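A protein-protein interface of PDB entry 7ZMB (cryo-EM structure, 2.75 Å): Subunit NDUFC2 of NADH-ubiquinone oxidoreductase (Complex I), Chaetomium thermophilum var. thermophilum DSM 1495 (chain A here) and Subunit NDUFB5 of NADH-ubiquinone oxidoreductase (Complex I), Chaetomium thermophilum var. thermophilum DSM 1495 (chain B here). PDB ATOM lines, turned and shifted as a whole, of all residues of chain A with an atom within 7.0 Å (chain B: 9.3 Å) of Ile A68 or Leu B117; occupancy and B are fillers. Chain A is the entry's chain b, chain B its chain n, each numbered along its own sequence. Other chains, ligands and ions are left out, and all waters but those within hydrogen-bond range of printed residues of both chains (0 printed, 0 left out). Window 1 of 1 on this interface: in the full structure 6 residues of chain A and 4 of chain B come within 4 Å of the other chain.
OE2 of Glu B122 is in salt-bridge range of NZ of Lys A71 (3.3 Å).
The backbone carbonyl oxygen (O) of Leu A61 lies within hydrogen-bond range of the side-chain amino group (NZ) of Lys A65 (2.9 Å). The side-chain amide oxygen (OE1) of Gln B110 lies close to the side-chain carboxylate (OD1) of Asp B114 (3.3 Å).
Arg A64 touches Leu B118. Asp B114 touches Lys A65 (CB to CD, 3.5 Å). Leu B117 touches Lys A65. CG of Lys A65 touches CD2 of Leu B118 (3.9 Å). CG2 of Ile A68 touches CG of Leu B117 (3.8 Å). CD1 of Ile A68 touches CD2 of Leu B118, at 3.9 Å. CG of Leu A69 touches CD2 of Leu B117 (3.8 Å).
Of the printed residues of chain B, Ile A68 touches Leu B117 and Leu B118. Leu B117 touches just these residues of chain A: Lys A65, Ile A68 and Leu A69. No residue of chain B comes within 4 Å of Ala A67. Leu A69 touches one residue of chain B. Of the printed residues of chain A, Asp B114 touches Lys A65 (3.5 Å). Of the printed residues of chain B, Arg A64 touches Leu B118 (3.8 Å). Printed residues of chain B within 4 Å of Lys A65: Asp B114, Leu B117 and Leu B118. Gln B110 touches none of the printed residues of chain A. The nearest printed residue of chain B that does not touch Ile A68 is Ala B121 (4.01 Å). The nearest printed residue of chain B that does not touch Arg A64 is Ala B121 (4.3 Å).
Of the 13 printed residues of chain A, 5 touch a printed residue of chain B.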
ATOM      1  N   LEU A  61      15.039 -19.691  14.447  1.00  0.00           N
ATOM      2  CA  LEU A  61      14.652 -18.887  13.292  1.00  0.00           C
ATOM      3  C   LEU A  61      13.962 -17.594  13.706  1.00  0.00           C
ATOM      4  O   LEU A  61      14.081 -16.583  13.010  1.00  0.00           O
ATOM      5  CB  LEU A  61      13.788 -19.704  12.333  1.00  0.00           C
ATOM      6  CG  LEU A  61      14.585 -20.842  11.704  1.00  0.00           C
ATOM      7  CD1 LEU A  61      13.720 -21.755  10.848  1.00  0.00           C
ATOM      8  CD2 LEU A  61      15.736 -20.279  10.891  1.00  0.00           C
ATOM      9  N   GLU A  63      14.825 -15.828  16.365  1.00  0.00           N
ATOM     10  CA  GLU A  63      15.963 -14.961  16.639  1.00  0.00           C
ATOM     11  C   GLU A  63      16.638 -14.511  15.353  1.00  0.00           C
ATOM     12  O   GLU A  63      16.998 -13.340  15.211  1.00  0.00           O
ATOM     13  CB  GLU A  63      16.971 -15.666  17.543  1.00  0.00           C
ATOM     14  CG  GLU A  63      16.400 -16.261  18.811  1.00  0.00           C
ATOM     15  CD  GLU A  63      17.281 -17.361  19.371  1.00  0.00           C
ATOM     16  OE1 GLU A  63      18.142 -17.871  18.624  1.00  0.00           O
ATOM     17  OE2 GLU A  63      17.140 -17.687  20.567  1.00  0.00           O
ATOM     18  N   ARG A  64      16.816 -15.430  14.406  1.00  0.00           N
ATOM     19  CA  ARG A  64      17.480 -15.086  13.155  1.00  0.00           C
ATOM     20  C   ARG A  64      16.689 -14.041  12.377  1.00  0.00           C
ATOM     21  O   ARG A  64      17.259 -13.063  11.889  1.00  0.00           O
ATOM     22  CB  ARG A  64      17.690 -16.347  12.315  1.00  0.00           C
ATOM     23  CG  ARG A  64      18.338 -16.106  10.977  1.00  0.00           C
ATOM     24  CD  ARG A  64      19.822 -15.877  11.124  1.00  0.00           C
ATOM     25  NE  ARG A  64      20.432 -15.313   9.923  1.00  0.00           N
ATOM     26  CZ  ARG A  64      21.010 -14.119   9.876  1.00  0.00           C
ATOM     27  NH1 ARG A  64      21.038 -13.355  10.952  1.00  0.00           N
ATOM     28  NH2 ARG A  64      21.548 -13.681   8.752  1.00  0.00           N
ATOM     29  N   LYS A  65      15.370 -14.220  12.262  1.00  0.00           N
ATOM     30  CA  LYS A  65      14.574 -13.248  11.517  1.00  0.00           C
ATOM     31  C   LYS A  65      14.626 -11.875  12.161  1.00  0.00           C
ATOM     32  O   LYS A  65      14.665 -10.864  11.454  1.00  0.00           O
ATOM     33  CB  LYS A  65      13.127 -13.722  11.353  1.00  0.00           C
ATOM     34  CG  LYS A  65      13.001 -14.990  10.509  1.00  0.00           C
ATOM     35  CD  LYS A  65      11.564 -15.418  10.283  1.00  0.00           C
ATOM     36  CE  LYS A  65      10.886 -15.959  11.529  1.00  0.00           C
ATOM     37  NZ  LYS A  65      11.483 -17.233  11.998  1.00  0.00           N
ATOM     38  N   GLN A  66      14.649 -11.814  13.490  1.00  0.00           N
ATOM     39  CA  GLN A  66      14.910 -10.544  14.155  1.00  0.00           C
ATOM     40  C   GLN A  66      16.305 -10.034  13.827  1.00  0.00           C
ATOM     41  O   GLN A  66      16.483  -8.864  13.475  1.00  0.00           O
ATOM     42  CB  GLN A  66      14.724 -10.697  15.659  1.00  0.00           C
ATOM     43  CG  GLN A  66      13.295 -10.985  16.062  1.00  0.00           C
ATOM     44  CD  GLN A  66      12.288 -10.431  15.074  1.00  0.00           C
ATOM     45  OE1 GLN A  66      11.663 -11.177  14.322  1.00  0.00           O
ATOM     46  NE2 GLN A  66      12.116  -9.112  15.081  1.00  0.00           N
ATOM     47  N   ALA A  67      17.303 -10.917  13.892  1.00  0.00           N
ATOM     48  CA  ALA A  67      18.678 -10.518  13.618  1.00  0.00           C
ATOM     49  C   ALA A  67      18.872 -10.053  12.181  1.00  0.00           C
ATOM     50  O   ALA A  67      19.773  -9.255  11.909  1.00  0.00           O
ATOM     51  CB  ALA A  67      19.623 -11.674  13.932  1.00  0.00           C
ATOM     52  N   ILE A  68      18.068 -10.552  11.243  1.00  0.00           N
ATOM     53  CA  ILE A  68      18.168 -10.078   9.867  1.00  0.00           C
ATOM     54  C   ILE A  68      17.593  -8.674   9.746  1.00  0.00           C
ATOM     55  O   ILE A  68      18.219  -7.780   9.166  1.00  0.00           O
ATOM     56  CB  ILE A  68      17.484 -11.059   8.901  1.00  0.00           C
ATOM     57  CG1 ILE A  68      18.212 -12.402   8.916  1.00  0.00           C
ATOM     58  CG2 ILE A  68      17.474 -10.489   7.507  1.00  0.00           C
ATOM     59  CD1 ILE A  68      17.547 -13.487   8.107  1.00  0.00           C
ATOM     60  N   LEU A  69      16.406  -8.450  10.316  1.00  0.00           N
ATOM     61  CA  LEU A  69      15.800  -7.124  10.287  1.00  0.00           C
ATOM     62  C   LEU A  69      16.697  -6.093  10.954  1.00  0.00           C
ATOM     63  O   LEU A  69      16.881  -4.991  10.431  1.00  0.00           O
ATOM     64  CB  LEU A  69      14.443  -7.144  10.985  1.00  0.00           C
ATOM     65  CG  LEU A  69      13.262  -7.893  10.385  1.00  0.00           C
ATOM     66  CD1 LEU A  69      12.395  -8.428  11.508  1.00  0.00           C
ATOM     67  CD2 LEU A  69      12.469  -6.983   9.477  1.00  0.00           C
ATOM     68  N   GLU A  70      17.255  -6.434  12.118  1.00  0.00           N
ATOM     69  CA  GLU A  70      18.124  -5.501  12.823  1.00  0.00           C
ATOM     70  C   GLU A  70      19.387  -5.208  12.026  1.00  0.00           C
ATOM     71  O   GLU A  70      19.846  -4.064  11.982  1.00  0.00           O
ATOM     72  CB  GLU A  70      18.475  -6.047  14.204  1.00  0.00           C
ATOM     73  CG  GLU A  70      17.489  -5.650  15.287  1.00  0.00           C
ATOM     74  CD  GLU A  70      18.055  -5.833  16.682  1.00  0.00           C
ATOM     75  OE1 GLU A  70      19.280  -6.048  16.802  1.00  0.00           O
ATOM     76  OE2 GLU A  70      17.277  -5.764  17.656  1.00  0.00           O
ATOM     77  N   LYS A  71      19.967  -6.229  11.399  1.00  0.00           N
ATOM     78  CA  LYS A  71      21.108  -5.993  10.523  1.00  0.00           C
ATOM     79  C   LYS A  71      20.729  -5.065   9.381  1.00  0.00           C
ATOM     80  O   LYS A  71      21.491  -4.162   9.025  1.00  0.00           O
ATOM     81  CB  LYS A  71      21.640  -7.319   9.984  1.00  0.00           C
ATOM     82  CG  LYS A  71      22.722  -7.159   8.946  1.00  0.00           C
ATOM     83  CD  LYS A  71      23.202  -8.497   8.427  1.00  0.00           C
ATOM     84  CE  LYS A  71      24.248  -8.309   7.345  1.00  0.00           C
ATOM     85  NZ  LYS A  71      23.697  -7.569   6.177  1.00  0.00           N
ATOM     86  N   ARG A  72      19.541  -5.265   8.810  1.00  0.00           N
ATOM     87  CA  ARG A  72      19.035  -4.450   7.714  1.00  0.00           C
ATOM     88  C   ARG A  72      18.560  -3.080   8.165  1.00  0.00           C
ATOM     89  O   ARG A  72      18.720  -2.105   7.423  1.00  0.00           O
ATOM     90  CB  ARG A  72      17.876  -5.166   7.013  1.00  0.00           C
ATOM     91  CG  ARG A  72      18.223  -6.534   6.441  1.00  0.00           C
ATOM     92  CD  ARG A  72      17.124  -7.023   5.516  1.00  0.00           C
ATOM     93  NE  ARG A  72      17.143  -6.284   4.258  1.00  0.00           N
ATOM     94  CZ  ARG A  72      16.246  -5.370   3.913  1.00  0.00           C
ATOM     95  NH1 ARG A  72      15.247  -5.079   4.725  1.00  0.00           N
ATOM     96  NH2 ARG A  72      16.354  -4.747   2.751  1.00  0.00           N
ATOM     97  N   ALA A  73      17.966  -2.989   9.357  1.00  0.00           N
ATOM     98  CA  ALA A  73      17.406  -1.720   9.808  1.00  0.00           C
ATOM     99  C   ALA A  73      18.499  -0.722  10.147  1.00  0.00           C
ATOM    100  O   ALA A  73      18.376   0.469   9.835  1.00  0.00           O
ATOM    101  CB  ALA A  73      16.492  -1.941  11.013  1.00  0.00           C
ATOM    102  N   ARG A  74      19.571  -1.178  10.793  1.00  0.00           N
ATOM    103  CA  ARG A  74      20.675  -0.281  11.101  1.00  0.00           C
ATOM    104  C   ARG A  74      21.545   0.006   9.888  1.00  0.00           C
ATOM    105  O   ARG A  74      22.306   0.978   9.908  1.00  0.00           O
ATOM    106  CB  ARG A  74      21.542  -0.853  12.224  1.00  0.00           C
ATOM    107  CG  ARG A  74      22.333  -2.080  11.838  1.00  0.00           C
ATOM    108  CD  ARG A  74      23.055  -2.667  13.034  1.00  0.00           C
ATOM    109  NE  ARG A  74      23.802  -3.870  12.684  1.00  0.00           N
ATOM    110  CZ  ARG A  74      24.507  -4.587  13.551  1.00  0.00           C
ATOM    111  NH1 ARG A  74      24.561  -4.222  14.824  1.00  0.00           N
ATOM    112  NH2 ARG A  74      25.157  -5.670  13.148  1.00  0.00           N
ATOM    113  N   GLU B 109       0.626 -14.936   4.329  1.00  0.00           N
ATOM    114  CA  GLU B 109       1.326 -13.688   4.049  1.00  0.00           C
ATOM    115  C   GLU B 109       2.557 -13.563   4.937  1.00  0.00           C
ATOM    116  O   GLU B 109       3.670 -13.319   4.459  1.00  0.00           O
ATOM    117  CB  GLU B 109       0.416 -12.485   4.292  1.00  0.00           C
ATOM    118  CG  GLU B 109      -0.788 -12.286   3.395  1.00  0.00           C
ATOM    119  CD  GLU B 109      -0.427 -11.961   1.965  1.00  0.00           C
ATOM    120  OE1 GLU B 109       0.621 -11.324   1.736  1.00  0.00           O
ATOM    121  OE2 GLU B 109      -1.238 -12.277   1.078  1.00  0.00           O
ATOM    122  N   GLN B 110       2.364 -13.729   6.246  1.00  0.00           N
ATOM    123  CA  GLN B 110       3.467 -13.553   7.179  1.00  0.00           C
ATOM    124  C   GLN B 110       4.550 -14.596   6.948  1.00  0.00           C
ATOM    125  O   GLN B 110       5.743 -14.271   6.949  1.00  0.00           O
ATOM    126  CB  GLN B 110       2.958 -13.608   8.617  1.00  0.00           C
ATOM    127  CG  GLN B 110       3.939 -13.045   9.623  1.00  0.00           C
ATOM    128  CD  GLN B 110       4.490 -11.697   9.202  1.00  0.00           C
ATOM    129  OE1 GLN B 110       5.570 -11.610   8.616  1.00  0.00           O
ATOM    130  NE2 GLN B 110       3.750 -10.636   9.500  1.00  0.00           N
ATOM    131  N   ALA B 111       4.152 -15.847   6.717  1.00  0.00           N
ATOM    132  CA  ALA B 111       5.127 -16.884   6.410  1.00  0.00           C
ATOM    133  C   ALA B 111       5.888 -16.563   5.134  1.00  0.00           C
ATOM    134  O   ALA B 111       7.103 -16.763   5.062  1.00  0.00           O
ATOM    135  CB  ALA B 111       4.435 -18.240   6.295  1.00  0.00           C
ATOM    136  N   ALA B 112       5.190 -16.053   4.118  1.00  0.00           N
ATOM    137  CA  ALA B 112       5.852 -15.705   2.864  1.00  0.00           C
ATOM    138  C   ALA B 112       6.887 -14.610   3.073  1.00  0.00           C
ATOM    139  O   ALA B 112       7.943 -14.614   2.435  1.00  0.00           O
ATOM    140  CB  ALA B 112       4.819 -15.276   1.825  1.00  0.00           C
ATOM    141  N   HIS B 113       6.594 -13.669   3.969  1.00  0.00           N
ATOM    142  CA  HIS B 113       7.550 -12.574   4.275  1.00  0.00           C
ATOM    143  C   HIS B 113       8.761 -13.141   5.017  1.00  0.00           C
ATOM    144  O   HIS B 113       9.881 -12.695   4.739  1.00  0.00           O
ATOM    145  CB  HIS B 113       6.864 -11.472   5.087  1.00  0.00           C
ATOM    146  CG  HIS B 113       7.820 -10.512   5.709  1.00  0.00           C
ATOM    147  ND1 HIS B 113       8.515  -9.578   4.967  1.00  0.00           N
ATOM    148  CD2 HIS B 113       8.208 -10.345   6.991  1.00  0.00           C
ATOM    149  CE1 HIS B 113       9.288  -8.874   5.767  1.00  0.00           C
ATOM    150  NE2 HIS B 113       9.117  -9.324   7.014  1.00  0.00           N
ATOM    151  N   ASP B 114       8.528 -14.072   5.942  1.00  0.00           N
ATOM    152  CA  ASP B 114       9.639 -14.655   6.688  1.00  0.00           C
ATOM    153  C   ASP B 114      10.588 -15.393   5.760  1.00  0.00           C
ATOM    154  O   ASP B 114      11.809 -15.239   5.851  1.00  0.00           O
ATOM    155  CB  ASP B 114       9.114 -15.593   7.774  1.00  0.00           C
ATOM    156  CG  ASP B 114       8.075 -14.936   8.659  1.00  0.00           C
ATOM    157  OD1 ASP B 114       8.132 -13.700   8.830  1.00  0.00           O
ATOM    158  OD2 ASP B 114       7.198 -15.656   9.181  1.00  0.00           O
ATOM    159  N   LYS B 115      10.036 -16.193   4.846  1.00  0.00           N
ATOM    160  CA  LYS B 115      10.867 -16.883   3.869  1.00  0.00           C
ATOM    161  C   LYS B 115      11.601 -15.887   2.991  1.00  0.00           C
ATOM    162  O   LYS B 115      12.784 -16.070   2.686  1.00  0.00           O
ATOM    163  CB  LYS B 115      10.004 -17.825   3.030  1.00  0.00           C
ATOM    164  CG  LYS B 115      10.692 -18.414   1.807  1.00  0.00           C
ATOM    165  CD  LYS B 115       9.775 -19.389   1.081  1.00  0.00           C
ATOM    166  CE  LYS B 115      10.178 -19.568  -0.376  1.00  0.00           C
ATOM    167  NZ  LYS B 115       9.542 -18.557  -1.273  1.00  0.00           N
ATOM    168  N   HIS B 116      10.923 -14.808   2.600  1.00  0.00           N
ATOM    169  CA  HIS B 116      11.562 -13.768   1.801  1.00  0.00           C
ATOM    170  C   HIS B 116      12.735 -13.143   2.548  1.00  0.00           C
ATOM    171  O   HIS B 116      13.787 -12.883   1.960  1.00  0.00           O
ATOM    172  CB  HIS B 116      10.515 -12.726   1.414  1.00  0.00           C
ATOM    173  CG  HIS B 116      11.078 -11.430   0.928  1.00  0.00           C
ATOM    174  ND1 HIS B 116      10.608 -10.210   1.364  1.00  0.00           N
ATOM    175  CD2 HIS B 116      12.053 -11.159   0.031  1.00  0.00           C
ATOM    176  CE1 HIS B 116      11.273  -9.245   0.761  1.00  0.00           C
ATOM    177  NE2 HIS B 116      12.158  -9.793  -0.050  1.00  0.00           N
ATOM    178  N   LEU B 117      12.576 -12.920   3.852  1.00  0.00           N
ATOM    179  CA  LEU B 117      13.676 -12.448   4.685  1.00  0.00           C
ATOM    180  C   LEU B 117      14.837 -13.436   4.719  1.00  0.00           C
ATOM    181  O   LEU B 117      16.002 -13.040   4.611  1.00  0.00           O
ATOM    182  CB  LEU B 117      13.162 -12.201   6.102  1.00  0.00           C
ATOM    183  CG  LEU B 117      13.726 -11.094   6.989  1.00  0.00           C
ATOM    184  CD1 LEU B 117      13.633  -9.756   6.339  1.00  0.00           C
ATOM    185  CD2 LEU B 117      12.980 -11.093   8.307  1.00  0.00           C
ATOM    186  N   LEU B 118      14.561 -14.686   5.078  1.00  0.00           N
ATOM    187  CA  LEU B 118      15.638 -15.692   5.249  1.00  0.00           C
ATOM    188  C   LEU B 118      16.341 -15.996   3.917  1.00  0.00           C
ATOM    189  O   LEU B 118      17.578 -16.097   3.923  1.00  0.00           O
ATOM    190  CB  LEU B 118      15.046 -16.943   5.904  1.00  0.00           C
ATOM    191  CG  LEU B 118      14.530 -16.781   7.332  1.00  0.00           C
ATOM    192  CD1 LEU B 118      13.441 -17.799   7.623  1.00  0.00           C
ATOM    193  CD2 LEU B 118      15.660 -16.912   8.338  1.00  0.00           C
ATOM    194  N   LEU B 119      15.596 -16.192   2.834  1.00  0.00           N
ATOM    195  CA  LEU B 119      16.202 -16.512   1.510  1.00  0.00           C
ATOM    196  C   LEU B 119      17.055 -15.356   0.980  1.00  0.00           C
ATOM    197  O   LEU B 119      18.077 -15.639   0.345  1.00  0.00           O
ATOM    198  CB  LEU B 119      15.120 -16.916   0.508  1.00  0.00           C
ATOM    199  CG  LEU B 119      15.198 -18.362   0.023  1.00  0.00           C
ATOM    200  CD1 LEU B 119      14.992 -19.328   1.177  1.00  0.00           C
ATOM    201  CD2 LEU B 119      14.178 -18.619  -1.075  1.00  0.00           C
ATOM    202  N   THR B 120      16.635 -14.109   1.190  1.00  0.00           N
ATOM    203  CA  THR B 120      17.361 -12.965   0.584  1.00  0.00           C
ATOM    204  C   THR B 120      18.355 -12.342   1.560  1.00  0.00           C
ATOM    205  O   THR B 120      18.773 -11.207   1.294  1.00  0.00           O
ATOM    206  CB  THR B 120      16.393 -11.892   0.080  1.00  0.00           C
ATOM    207  OG1 THR B 120      15.752 -11.330   1.224  1.00  0.00           O
ATOM    208  CG2 THR B 120      15.371 -12.424  -0.899  1.00  0.00           C
ATOM    209  N   ALA B 121      18.747 -13.059   2.615  1.00  0.00           N
ATOM    210  CA  ALA B 121      19.722 -12.543   3.602  1.00  0.00           C
ATOM    211  C   ALA B 121      21.094 -12.402   2.950  1.00  0.00           C
ATOM    212  O   ALA B 121      21.488 -13.297   2.197  1.00  0.00           O
ATOM    213  CB  ALA B 121      19.785 -13.456   4.785  1.00  0.00           C
ATOM    214  N   GLU B 122      21.801 -11.317   3.253  1.00  0.00           N
ATOM    215  CA  GLU B 122      23.113 -11.050   2.608  1.00  0.00           C
ATOM    216  C   GLU B 122      24.148 -12.109   2.984  1.00  0.00           C
ATOM    217  O   GLU B 122      24.161 -12.536   4.151  1.00  0.00           O
ATOM    218  CB  GLU B 122      23.619  -9.668   3.015  1.00  0.00           C
ATOM    219  CG  GLU B 122      22.639  -8.555   2.696  1.00  0.00           C
ATOM    220  CD  GLU B 122      23.156  -7.153   2.971  1.00  0.00           C
ATOM    221  OE1 GLU B 122      22.325  -6.233   3.101  1.00  0.00           O
ATOM    222  OE2 GLU B 122      24.390  -6.985   3.052  1.00  0.00           O
